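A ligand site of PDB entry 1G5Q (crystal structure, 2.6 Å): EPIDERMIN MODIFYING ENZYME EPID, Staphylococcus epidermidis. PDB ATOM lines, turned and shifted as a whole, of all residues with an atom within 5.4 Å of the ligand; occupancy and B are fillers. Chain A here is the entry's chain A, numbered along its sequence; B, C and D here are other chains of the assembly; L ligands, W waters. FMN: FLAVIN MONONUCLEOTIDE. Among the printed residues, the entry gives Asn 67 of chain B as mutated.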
ATOM      1  N   THR A  10      21.399   5.005 -27.682  1.00  0.00           N
ATOM      2  CA  THR A  10      22.523   4.402 -26.984  1.00  0.00           C
ATOM      3  C   THR A  10      22.116   3.782 -25.640  1.00  0.00           C
ATOM      4  O   THR A  10      20.972   3.927 -25.195  1.00  0.00           O
ATOM      5  CB  THR A  10      23.682   5.413 -26.783  1.00  0.00           C
ATOM      6  OG1 THR A  10      23.297   6.411 -25.830  1.00  0.00           O
ATOM      7  CG2 THR A  10      24.026   6.075 -28.118  1.00  0.00           C
ATOM      8  N   ALA A  11      23.066   3.107 -24.992  1.00  0.00           N
ATOM      9  CA  ALA A  11      22.805   2.400 -23.741  1.00  0.00           C
ATOM     10  C   ALA A  11      22.567   3.191 -22.459  1.00  0.00           C
ATOM     11  O   ALA A  11      23.304   3.059 -21.474  1.00  0.00           O
ATOM     12  CB  ALA A  11      23.911   1.367 -23.508  1.00  0.00           C
ATOM     13  N   SER A  12      21.520   4.005 -22.480  1.00  0.00           N
ATOM     14  CA  SER A  12      21.137   4.761 -21.300  1.00  0.00           C
ATOM     15  C   SER A  12      19.937   3.996 -20.771  1.00  0.00           C
ATOM     16  O   SER A  12      19.169   3.435 -21.541  1.00  0.00           O
ATOM     17  CB  SER A  12      20.719   6.176 -21.667  1.00  0.00           C
ATOM     18  OG  SER A  12      19.873   6.703 -20.658  1.00  0.00           O
ATOM     19  N   ILE A  13      19.761   3.965 -19.446  1.00  0.00           N
ATOM     20  CA  ILE A  13      18.624   3.259 -18.866  1.00  0.00           C
ATOM     21  C   ILE A  13      17.323   3.716 -19.516  1.00  0.00           C
ATOM     22  O   ILE A  13      16.363   2.950 -19.624  1.00  0.00           O
ATOM     23  CB  ILE A  13      18.545   3.490 -17.330  1.00  0.00           C
ATOM     24  CG1 ILE A  13      17.345   2.747 -16.750  1.00  0.00           C
ATOM     25  CG2 ILE A  13      18.477   4.978 -17.023  1.00  0.00           C
ATOM     26  CD1 ILE A  13      17.384   1.243 -16.954  1.00  0.00           C
ATOM     27  N   ASN A  14      17.300   4.959 -19.982  1.00  0.00           N
ATOM     28  CA  ASN A  14      16.088   5.504 -20.599  1.00  0.00           C
ATOM     29  C   ASN A  14      15.772   5.007 -22.008  1.00  0.00           C
ATOM     30  O   ASN A  14      14.721   5.328 -22.558  1.00  0.00           O
ATOM     31  CB  ASN A  14      16.157   7.035 -20.582  1.00  0.00           C
ATOM     32  CG  ASN A  14      16.004   7.591 -19.178  1.00  0.00           C
ATOM     33  OD1 ASN A  14      14.932   7.491 -18.563  1.00  0.00           O
ATOM     34  ND2 ASN A  14      17.088   8.159 -18.644  1.00  0.00           N
ATOM     35  N   SER A  37      23.045   1.148 -30.440  1.00  0.00           N
ATOM     36  CA  SER A  37      24.443   0.848 -30.158  1.00  0.00           C
ATOM     37  C   SER A  37      24.391  -0.624 -29.729  1.00  0.00           C
ATOM     38  O   SER A  37      23.363  -1.098 -29.243  1.00  0.00           O
ATOM     39  CB  SER A  37      24.968   1.719 -29.012  1.00  0.00           C
ATOM     40  OG  SER A  37      24.364   1.393 -27.757  1.00  0.00           O
ATOM     41  N   PRO A  38      25.503  -1.362 -29.898  1.00  0.00           N
ATOM     42  CA  PRO A  38      25.502  -2.777 -29.491  1.00  0.00           C
ATOM     43  C   PRO A  38      25.040  -3.011 -28.047  1.00  0.00           C
ATOM     44  O   PRO A  38      24.259  -3.918 -27.791  1.00  0.00           O
ATOM     45  CB  PRO A  38      26.945  -3.193 -29.720  1.00  0.00           C
ATOM     46  CG  PRO A  38      27.344  -2.358 -30.902  1.00  0.00           C
ATOM     47  CD  PRO A  38      26.768  -1.009 -30.569  1.00  0.00           C
ATOM     48  N   SER A  39      25.520  -2.187 -27.128  1.00  0.00           N
ATOM     49  CA  SER A  39      25.190  -2.314 -25.709  1.00  0.00           C
ATOM     50  C   SER A  39      23.729  -2.072 -25.323  1.00  0.00           C
ATOM     51  O   SER A  39      23.249  -2.641 -24.348  1.00  0.00           O
ATOM     52  CB  SER A  39      26.059  -1.343 -24.879  1.00  0.00           C
ATOM     53  OG  SER A  39      27.432  -1.653 -24.991  1.00  0.00           O
ATOM     54  N   SER A  40      23.030  -1.233 -26.067  1.00  0.00           N
ATOM     55  CA  SER A  40      21.646  -0.949 -25.722  1.00  0.00           C
ATOM     56  C   SER A  40      20.762  -2.178 -25.865  1.00  0.00           C
ATOM     57  O   SER A  40      19.654  -2.221 -25.331  1.00  0.00           O
ATOM     58  CB  SER A  40      21.112   0.229 -26.558  1.00  0.00           C
ATOM     59  OG  SER A  40      21.314   0.012 -27.938  1.00  0.00           O
ATOM     60  N   PHE A  43      19.300  -3.790 -22.796  1.00  0.00           N
ATOM     61  CA  PHE A  43      18.217  -3.122 -22.100  1.00  0.00           C
ATOM     62  C   PHE A  43      16.858  -3.423 -22.697  1.00  0.00           C
ATOM     63  O   PHE A  43      15.857  -3.441 -21.979  1.00  0.00           O
ATOM     64  CB  PHE A  43      18.409  -1.611 -22.121  1.00  0.00           C
ATOM     65  CG  PHE A  43      19.589  -1.123 -21.352  1.00  0.00           C
ATOM     66  CD1 PHE A  43      20.888  -1.347 -21.811  1.00  0.00           C
ATOM     67  CD2 PHE A  43      19.424  -0.416 -20.164  1.00  0.00           C
ATOM     68  CE1 PHE A  43      21.984  -0.865 -21.108  1.00  0.00           C
ATOM     69  CE2 PHE A  43      20.510   0.064 -19.462  1.00  0.00           C
ATOM     70  CZ  PHE A  43      21.801  -0.161 -19.937  1.00  0.00           C
ATOM     71  N   ALA A  82      21.597  10.047 -25.540  1.00  0.00           N
ATOM     72  CA  ALA A  82      23.009  10.025 -25.881  1.00  0.00           C
ATOM     73  C   ALA A  82      23.810   9.753 -24.616  1.00  0.00           C
ATOM     74  O   ALA A  82      23.761  10.513 -23.649  1.00  0.00           O
ATOM     75  CB  ALA A  82      23.427  11.355 -26.488  1.00  0.00           C
ATOM     76  N   SER A  83      24.548   8.646 -24.624  1.00  0.00           N
ATOM     77  CA  SER A  83      25.371   8.257 -23.482  1.00  0.00           C
ATOM     78  C   SER A  83      26.686   9.016 -23.472  1.00  0.00           C
ATOM     79  O   SER A  83      27.133   9.534 -24.495  1.00  0.00           O
ATOM     80  CB  SER A  83      25.671   6.758 -23.529  1.00  0.00           C
ATOM     81  OG  SER A  83      26.492   6.429 -24.648  1.00  0.00           O
ATOM     82  N   ALA A  84      27.303   9.072 -22.294  1.00  0.00           N
ATOM     83  CA  ALA A  84      28.584   9.742 -22.156  1.00  0.00           C
ATOM     84  C   ALA A  84      29.583   9.121 -23.123  1.00  0.00           C
ATOM     85  O   ALA A  84      30.331   9.820 -23.816  1.00  0.00           O
ATOM     86  CB  ALA A  84      29.085   9.600 -20.719  1.00  0.00           C
ATOM     87  N   ASN A  85      29.584   7.789 -23.175  1.00  0.00           N
ATOM     88  CA  ASN A  85      30.495   7.058 -24.041  1.00  0.00           C
ATOM     89  C   ASN A  85      30.372   7.447 -25.507  1.00  0.00           C
ATOM     90  O   ASN A  85      31.373   7.763 -26.150  1.00  0.00           O
ATOM     91  CB  ASN A  85      30.286   5.557 -23.894  1.00  0.00           C
ATOM     92  CG  ASN A  85      31.097   4.751 -24.909  1.00  0.00           C
ATOM     93  OD1 ASN A  85      30.529   4.102 -25.795  1.00  0.00           O
ATOM     94  ND2 ASN A  85      32.416   4.812 -24.794  1.00  0.00           N
ATOM     95  N   THR A  86      29.146   7.419 -26.045  1.00  0.00           N
ATOM     96  CA  THR A  86      28.944   7.766 -27.456  1.00  0.00           C
ATOM     97  C   THR A  86      29.258   9.236 -27.736  1.00  0.00           C
ATOM     98  O   THR A  86      29.797   9.566 -28.791  1.00  0.00           O
ATOM     99  CB  THR A  86      27.499   7.451 -27.914  1.00  0.00           C
ATOM    100  OG1 THR A  86      27.353   6.025 -28.027  1.00  0.00           O
ATOM    101  CG2 THR A  86      27.201   8.080 -29.269  1.00  0.00           C
ATOM    102  N   ASN A  97      31.529   1.171 -34.347  1.00  0.00           N
ATOM    103  CA  ASN A  97      30.256   0.474 -34.500  1.00  0.00           C
ATOM    104  C   ASN A  97      29.456   1.297 -35.504  1.00  0.00           C
ATOM    105  O   ASN A  97      29.819   2.444 -35.790  1.00  0.00           O
ATOM    106  CB  ASN A  97      29.493   0.299 -33.172  1.00  0.00           C
ATOM    107  CG  ASN A  97      29.178   1.599 -32.479  1.00  0.00           C
ATOM    108  OD1 ASN A  97      28.814   2.585 -33.117  1.00  0.00           O
ATOM    109  ND2 ASN A  97      29.275   1.599 -31.159  1.00  0.00           N
ATOM    110  N   ASN A 115      22.085  12.133 -21.717  1.00  0.00           N
ATOM    111  CA  ASN A 115      21.330  11.560 -20.608  1.00  0.00           C
ATOM    112  C   ASN A 115      22.270  10.686 -19.804  1.00  0.00           C
ATOM    113  O   ASN A 115      22.890   9.757 -20.331  1.00  0.00           O
ATOM    114  CB  ASN A 115      20.148  10.735 -21.090  1.00  0.00           C
ATOM    115  CG  ASN A 115      19.269  10.270 -19.940  1.00  0.00           C
ATOM    116  OD1 ASN A 115      19.457   9.169 -19.409  1.00  0.00           O
ATOM    117  ND2 ASN A 115      18.330  11.114 -19.514  1.00  0.00           N
ATOM    118  N   MET A 116      22.386  11.003 -18.521  1.00  0.00           N
ATOM    119  CA  MET A 116      23.268  10.281 -17.626  1.00  0.00           C
ATOM    120  C   MET A 116      23.146  10.889 -16.245  1.00  0.00           C
ATOM    121  O   MET A 116      22.512  11.926 -16.093  1.00  0.00           O
ATOM    122  CB  MET A 116      24.713  10.443 -18.099  1.00  0.00           C
ATOM    123  CG  MET A 116      25.181  11.897 -18.057  1.00  0.00           C
ATOM    124  SD  MET A 116      26.764  12.190 -18.845  1.00  0.00           S
ATOM    125  CE  MET A 116      26.265  12.291 -20.567  1.00  0.00           C
ATOM    126  N   ASN A 117      23.750  10.243 -15.263  1.00  0.00           N
ATOM    127  CA  ASN A 117      23.727  10.752 -13.896  1.00  0.00           C
ATOM    128  C   ASN A 117      24.477  12.071 -13.857  1.00  0.00           C
ATOM    129  O   ASN A 117      25.457  12.267 -14.592  1.00  0.00           O
ATOM    130  CB  ASN A 117      24.415   9.778 -12.945  1.00  0.00           C
ATOM    131  CG  ASN A 117      23.422   9.032 -12.095  1.00  0.00           C
ATOM    132  OD1 ASN A 117      22.625   8.257 -12.605  1.00  0.00           O
ATOM    133  ND2 ASN A 117      23.474   9.261 -10.779  1.00  0.00           N
ATOM    134  N   MET A 120      28.155  11.728 -13.581  1.00  0.00           N
ATOM    135  CA  MET A 120      28.874  11.404 -14.810  1.00  0.00           C
ATOM    136  C   MET A 120      28.996  12.685 -15.629  1.00  0.00           C
ATOM    137  O   MET A 120      30.038  12.953 -16.242  1.00  0.00           O
ATOM    138  CB  MET A 120      28.116  10.350 -15.610  1.00  0.00           C
ATOM    139  CG  MET A 120      27.958   9.010 -14.904  1.00  0.00           C
ATOM    140  SD  MET A 120      26.869   7.868 -15.792  1.00  0.00           S
ATOM    141  CE  MET A 120      27.936   7.310 -17.120  1.00  0.00           C
ATOM    142  N   ILE A 151      17.107   4.545  -9.970  1.00  0.00           N
ATOM    143  CA  ILE A 151      16.952   3.136  -9.678  1.00  0.00           C
ATOM    144  C   ILE A 151      17.718   2.609  -8.468  1.00  0.00           C
ATOM    145  O   ILE A 151      17.263   1.669  -7.830  1.00  0.00           O
ATOM    146  CB  ILE A 151      17.286   2.281 -10.938  1.00  0.00           C
ATOM    147  CG1 ILE A 151      18.703   2.567 -11.438  1.00  0.00           C
ATOM    148  CG2 ILE A 151      16.270   2.593 -12.046  1.00  0.00           C
ATOM    149  CD1 ILE A 151      19.042   1.889 -12.762  1.00  0.00           C
ATOM    150  N   PRO B  63      25.073  -8.290 -17.314  1.00  0.00           N
ATOM    151  CA  PRO B  63      25.259  -7.145 -18.209  1.00  0.00           C
ATOM    152  C   PRO B  63      24.625  -5.849 -17.706  1.00  0.00           C
ATOM    153  O   PRO B  63      24.871  -4.772 -18.262  1.00  0.00           O
ATOM    154  CB  PRO B  63      24.591  -7.613 -19.513  1.00  0.00           C
ATOM    155  CG  PRO B  63      24.582  -9.108 -19.401  1.00  0.00           C
ATOM    156  CD  PRO B  63      24.253  -9.331 -17.963  1.00  0.00           C
ATOM    157  N   LEU B  64      23.811  -5.940 -16.658  1.00  0.00           N
ATOM    158  CA  LEU B  64      23.159  -4.750 -16.132  1.00  0.00           C
ATOM    159  C   LEU B  64      23.630  -4.273 -14.764  1.00  0.00           C
ATOM    160  O   LEU B  64      22.845  -3.772 -13.963  1.00  0.00           O
ATOM    161  CB  LEU B  64      21.645  -4.961 -16.117  1.00  0.00           C
ATOM    162  CG  LEU B  64      21.036  -5.202 -17.514  1.00  0.00           C
ATOM    163  CD1 LEU B  64      19.557  -5.479 -17.397  1.00  0.00           C
ATOM    164  CD2 LEU B  64      21.286  -3.991 -18.392  1.00  0.00           C
ATOM    165  N   LEU B  65      24.933  -4.421 -14.515  1.00  0.00           N
ATOM    166  CA  LEU B  65      25.530  -3.978 -13.270  1.00  0.00           C
ATOM    167  C   LEU B  65      25.491  -2.429 -13.250  1.00  0.00           C
ATOM    168  O   LEU B  65      25.873  -1.760 -14.211  1.00  0.00           O
ATOM    169  CB  LEU B  65      26.977  -4.467 -13.188  1.00  0.00           C
ATOM    170  CG  LEU B  65      27.398  -5.501 -12.132  1.00  0.00           C
ATOM    171  CD1 LEU B  65      26.202  -6.271 -11.624  1.00  0.00           C
ATOM    172  CD2 LEU B  65      28.434  -6.443 -12.743  1.00  0.00           C
ATOM    173  N   ASN B  66      25.000  -1.881 -12.138  1.00  0.00           N
ATOM    174  CA  ASN B  66      24.876  -0.442 -11.961  1.00  0.00           C
ATOM    175  C   ASN B  66      26.222   0.207 -11.624  1.00  0.00           C
ATOM    176  O   ASN B  66      26.702   0.083 -10.495  1.00  0.00           O
ATOM    177  CB  ASN B  66      23.872  -0.173 -10.835  1.00  0.00           C
ATOM    178  CG  ASN B  66      23.454   1.282 -10.745  1.00  0.00           C
ATOM    179  OD1 ASN B  66      24.282   2.193 -10.875  1.00  0.00           O
ATOM    180  ND2 ASN B  66      22.168   1.511 -10.498  1.00  0.00           N
ATOM    181  N   ASN B  67      26.827   0.894 -12.582  1.00  0.00           N
ATOM    182  CA  ASN B  67      28.128   1.525 -12.357  1.00  0.00           C
ATOM    183  C   ASN B  67      28.105   2.581 -11.249  1.00  0.00           C
ATOM    184  O   ASN B  67      29.118   2.833 -10.599  1.00  0.00           O
ATOM    185  CB  ASN B  67      28.677   2.135 -13.644  1.00  0.00           C
ATOM    186  CG  ASN B  67      27.753   3.187 -14.241  1.00  0.00           C
ATOM    187  OD1 ASN B  67      26.676   2.868 -14.737  1.00  0.00           O
ATOM    188  ND2 ASN B  67      28.170   4.454 -14.167  1.00  0.00           N
ATOM    189  N   CYS B  95      34.057   5.031 -22.512  1.00  0.00           N
ATOM    190  CA  CYS B  95      33.652   3.971 -21.602  1.00  0.00           C
ATOM    191  C   CYS B  95      32.759   2.956 -22.301  1.00  0.00           C
ATOM    192  O   CYS B  95      31.537   2.931 -22.077  1.00  0.00           O
ATOM    193  CB  CYS B  95      32.929   4.578 -20.399  1.00  0.00           C
ATOM    194  SG  CYS B  95      31.851   5.990 -20.780  1.00  0.00           S
ATOM    195  N   ASP B  96      33.370   2.114 -23.125  1.00  0.00           N
ATOM    196  CA  ASP B  96      32.626   1.100 -23.858  1.00  0.00           C
ATOM    197  C   ASP B  96      32.646  -0.298 -23.220  1.00  0.00           C
ATOM    198  O   ASP B  96      32.353  -1.290 -23.876  1.00  0.00           O
ATOM    199  CB  ASP B  96      33.091   1.028 -25.312  1.00  0.00           C
ATOM    200  CG  ASP B  96      34.583   1.010 -25.459  1.00  0.00           C
ATOM    201  OD1 ASP B  96      35.295   0.762 -24.459  1.00  0.00           O
ATOM    202  OD2 ASP B  96      35.054   1.229 -26.589  1.00  0.00           O
ATOM    203  N   ASN B  97      33.008  -0.350 -21.945  1.00  0.00           N
ATOM    204  CA  ASN B  97      32.962  -1.583 -21.173  1.00  0.00           C
ATOM    205  C   ASN B  97      32.724  -1.165 -19.726  1.00  0.00           C
ATOM    206  O   ASN B  97      32.875   0.006 -19.386  1.00  0.00           O
ATOM    207  CB  ASN B  97      34.237  -2.448 -21.322  1.00  0.00           C
ATOM    208  CG  ASN B  97      35.494  -1.742 -20.872  1.00  0.00           C
ATOM    209  OD1 ASN B  97      35.503  -1.020 -19.879  1.00  0.00           O
ATOM    210  ND2 ASN B  97      36.577  -1.973 -21.596  1.00  0.00           N
ATOM    211  N   THR B 101      33.609   2.424 -17.767  1.00  0.00           N
ATOM    212  CA  THR B 101      32.408   3.167 -17.379  1.00  0.00           C
ATOM    213  C   THR B 101      32.525   3.520 -15.903  1.00  0.00           C
ATOM    214  O   THR B 101      32.175   4.632 -15.497  1.00  0.00           O
ATOM    215  CB  THR B 101      31.134   2.339 -17.593  1.00  0.00           C
ATOM    216  OG1 THR B 101      30.965   2.075 -18.986  1.00  0.00           O
ATOM    217  CG2 THR B 101      29.916   3.084 -17.058  1.00  0.00           C
ATOM    218  N   CYS C   5      20.532   6.332 -12.737  1.00  0.00           N
ATOM    219  CA  CYS C   5      21.168   5.223 -12.045  1.00  0.00           C
ATOM    220  C   CYS C   5      21.451   5.588 -10.594  1.00  0.00           C
ATOM    221  O   CYS C   5      21.035   4.794  -9.711  1.00  0.00           O
ATOM    222  CB  CYS C   5      22.474   4.828 -12.737  1.00  0.00           C
ATOM    223  SG  CYS C   5      22.252   3.597 -14.033  1.00  0.00           S
ATOM    224  OXT CYS C   5      22.078   6.636 -10.356  1.00  0.00           O
ATOM    225  N   LEU D  51      15.822  -4.149 -12.273  1.00  0.00           N
ATOM    226  CA  LEU D  51      16.257  -2.858 -11.777  1.00  0.00           C
ATOM    227  C   LEU D  51      15.129  -2.041 -11.180  1.00  0.00           C
ATOM    228  O   LEU D  51      15.374  -1.024 -10.522  1.00  0.00           O
ATOM    229  CB  LEU D  51      16.896  -2.052 -12.919  1.00  0.00           C
ATOM    230  CG  LEU D  51      18.133  -2.690 -13.577  1.00  0.00           C
ATOM    231  CD1 LEU D  51      18.528  -1.842 -14.758  1.00  0.00           C
ATOM    232  CD2 LEU D  51      19.276  -2.795 -12.576  1.00  0.00           C
HETATM  233  N1  FMN L   1      25.529   5.564 -19.493  1.00  0.00           N
HETATM  234  C2  FMN L   1      25.120   6.828 -19.800  1.00  0.00           C
HETATM  235  O2  FMN L   1      25.799   7.632 -20.390  1.00  0.00           O
HETATM  236  N3  FMN L   1      23.819   7.255 -19.391  1.00  0.00           N
HETATM  237  C4  FMN L   1      22.930   6.500 -18.708  1.00  0.00           C
HETATM  238  O4  FMN L   1      21.832   6.978 -18.375  1.00  0.00           O
HETATM  239  C4A FMN L   1      23.374   5.150 -18.350  1.00  0.00           C
HETATM  240  N5  FMN L   1      22.567   4.299 -17.718  1.00  0.00           N
HETATM  241  C5A FMN L   1      22.948   3.000 -17.544  1.00  0.00           C
HETATM  242  C6  FMN L   1      22.032   2.050 -16.927  1.00  0.00           C
HETATM  243  C7  FMN L   1      22.389   0.774 -16.597  1.00  0.00           C
HETATM  244  C7M FMN L   1      21.383  -0.199 -15.962  1.00  0.00           C
HETATM  245  C8  FMN L   1      23.673   0.248 -17.090  1.00  0.00           C
HETATM  246  C8M FMN L   1      24.063  -1.194 -16.876  1.00  0.00           C
HETATM  247  C9  FMN L   1      24.574   1.143 -17.646  1.00  0.00           C
HETATM  248  C9A FMN L   1      24.270   2.505 -17.896  1.00  0.00           C
HETATM  249  N10 FMN L   1      25.148   3.468 -18.481  1.00  0.00           N
HETATM  250  C10 FMN L   1      24.729   4.744 -18.817  1.00  0.00           C
HETATM  251  C1' FMN L   1      26.519   3.057 -18.896  1.00  0.00           C
HETATM  252  C2' FMN L   1      26.520   2.705 -20.402  1.00  0.00           C
HETATM  253  O2' FMN L   1      25.603   1.667 -20.763  1.00  0.00           O
HETATM  254  C3' FMN L   1      27.928   2.275 -20.828  1.00  0.00           C
HETATM  255  O3' FMN L   1      28.849   3.373 -20.635  1.00  0.00           O
HETATM  256  C4' FMN L   1      28.041   1.768 -22.263  1.00  0.00           C
HETATM  257  O4' FMN L   1      29.364   1.220 -22.510  1.00  0.00           O
HETATM  258  C5' FMN L   1      27.724   2.804 -23.329  1.00  0.00           C
HETATM  259  O5' FMN L   1      27.723   2.188 -24.617  1.00  0.00           O
HETATM  260  P   FMN L   1      27.044   2.817 -25.906  1.00  0.00           P
HETATM  261  O1P FMN L   1      27.676   4.154 -26.135  1.00  0.00           O
HETATM  262  O2P FMN L   1      25.573   2.891 -25.705  1.00  0.00           O
HETATM  263  O3P FMN L   1      27.413   1.795 -27.025  1.00  0.00           O
HETATM  264  O   HOH W   1      25.813  -1.093 -20.677  1.00  0.00           O
HETATM  265  O   HOH W   2      27.758  -0.634 -27.825  1.00  0.00           O
HETATM  266  O   HOH W   3      29.683   0.175 -25.122  1.00  0.00           O
HETATM  267  O   HOH W   4      30.342   1.908 -27.690  1.00  0.00           O
HETATM  268  O   HOH W   5      28.206   6.037 -21.076  1.00  0.00           O
HETATM  269  O   HOH W   6      28.161   3.414 -29.132  1.00  0.00           O
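The backbone NH of Ala 11 is in hydrogen-bond range of an oxygen (O2P) of the ligand.
O of Ala 11 is in hydrogen-bond range of O2' of the ligand, at 2.8 Å.
O1P of the ligand lies within hydrogen-bond range of OG1 of Thr 86, 2.7 Å away.
An oxygen (O4') of the ligand is in hydrogen-bond range of the backbone carbonyl oxygen (O) of Cys 95 of chain B (2.8 Å).
OG of Ser 37 is in hydrogen-bond range of O2P of the ligand.
N of Ala 84 sits at hydrogen-bond distance from O2 of the ligand.
The backbone carbonyl oxygen (O) of Asn 115 lies within hydrogen-bond range of a nitrogen (N3) of the ligand.
O4 of the ligand sits close to OD1 of Asn 115 (3.4 Å).
The side-chain amide oxygen (OD1) of Asn 85 sits close to an oxygen (O1P) of the ligand, at 2.9 Å.
The side-chain hydroxyl (OG) of Ser 83 is in hydrogen-bond range of an oxygen (O1P) of the ligand.
An oxygen (O3') of the ligand sits at hydrogen-bond distance from the side-chain hydroxyl (OG1) of Thr 101 of chain B (3.0 Å).
The side-chain hydroxyl (OG) of Ser 12 lies within hydrogen-bond range of an oxygen (O4) of the ligand.
The side-chain sulfur of Cys 5 of chain C sits close to a nitrogen (N5) of the ligand.
A nitrogen (N5) of the ligand sits at hydrogen-bond distance from the backbone NH (N) of Ile 13 (3.3 Å).
The side-chain amide nitrogen (ND2) of Asn 85 sits close to the backbone NH (N) of Cys 95 of chain B (2.8 Å).
O of Cys 95 of chain B sits at hydrogen-bond distance from OG1 of Thr 101 of chain B (3.3 Å).
The backbone carbonyl oxygen of Ser 37 lies within hydrogen-bond range of the side-chain hydroxyl of Ser 40.
The side-chain amide oxygen (OD1) of Asn 115 sits at hydrogen-bond distance from the side-chain hydroxyl (OG) of Ser 12, 2.8 Å away.
The backbone NH of Asn 115 lies within hydrogen-bond range of the backbone carbonyl oxygen of Ala 82 (3.0 Å).
The side-chain amide nitrogen of Asn 14 is in hydrogen-bond range of the side-chain amide oxygen of Asn 115 (2.7 Å).
The backbone NH (N) of Asp 96 of chain B lies close to the side-chain amide nitrogen (ND2) of Asn 85.
The backbone NH (N) of Asn 14 lies close to the side-chain hydroxyl (OG) of Ser 12 (3.2 Å).
Residues that only touch the ligand: Leu 65 of chain B (3.3 Å), Thr 10 (3.3 Å), Phe 43 (3.4 Å), Leu 51 of chain D (3.5 Å), Asp 96 of chain B (3.5 Å), Met 116 (3.5 Å), Leu 64 of chain B (3.7 Å), Met 120 (3.8 Å), Ser 39 (3.9 Å), Pro 63 of chain B (3.9 Å) and Asn 67 of chain B (3.98 Å).
Hydrophobic or aromatic side chains that line the ligand: Ala 11, Ile 13, Phe 43, Ala 84, Met 116, Met 120 and Leu 51 of chain D.
Within 4 Å of the ligand: Thr 10, Ala 11, Ser 12, Ile 13, Ser 37, Ser 39, Phe 43, Ser 83, Ala 84, Asn 85, Thr 86, Asn 115, Met 116, Met 120, Pro 63 of chain B, Leu 64 of chain B, Leu 65 of chain B, Asn 67 of chain B, Cys 95 of chain B, Asp 96 of chain B, Thr 101 of chain B, Cys 5 of chain C and Leu 51 of chain D.
The nearest printed residue that does not touch the ligand is Asn 97 of chain B (4.01 Å).
Water W2 bridges O3P of the ligand (2.6 Å) and N of Ser 39 (2.8 Å).
Water W6 lies within hydrogen-bond range of an oxygen (O3P) of the ligand, the side-chain amide nitrogen of Asn 97 of chain A and the side-chain hydroxyl of Thr 86.
Water W5 lies within hydrogen-bond range of an oxygen (O3') of the ligand (2.8 Å), the backbone NH (N) of Asn 85 (3.1 Å), the backbone NH (N) of Ala 84 (3.4 Å) and the side-chain sulfur (SG) of Cys 95 of chain B (3.7 Å).
Water W3 lies within hydrogen-bond range of O4' of the ligand (2.8 Å), OG of Ser 39 (2.9 Å) and O of Asp 96 of chain B (3.3 Å).
Water W4 bridges OD1 of Asn 85 (2.9 Å) and O3P of the ligand (3.0 Å).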
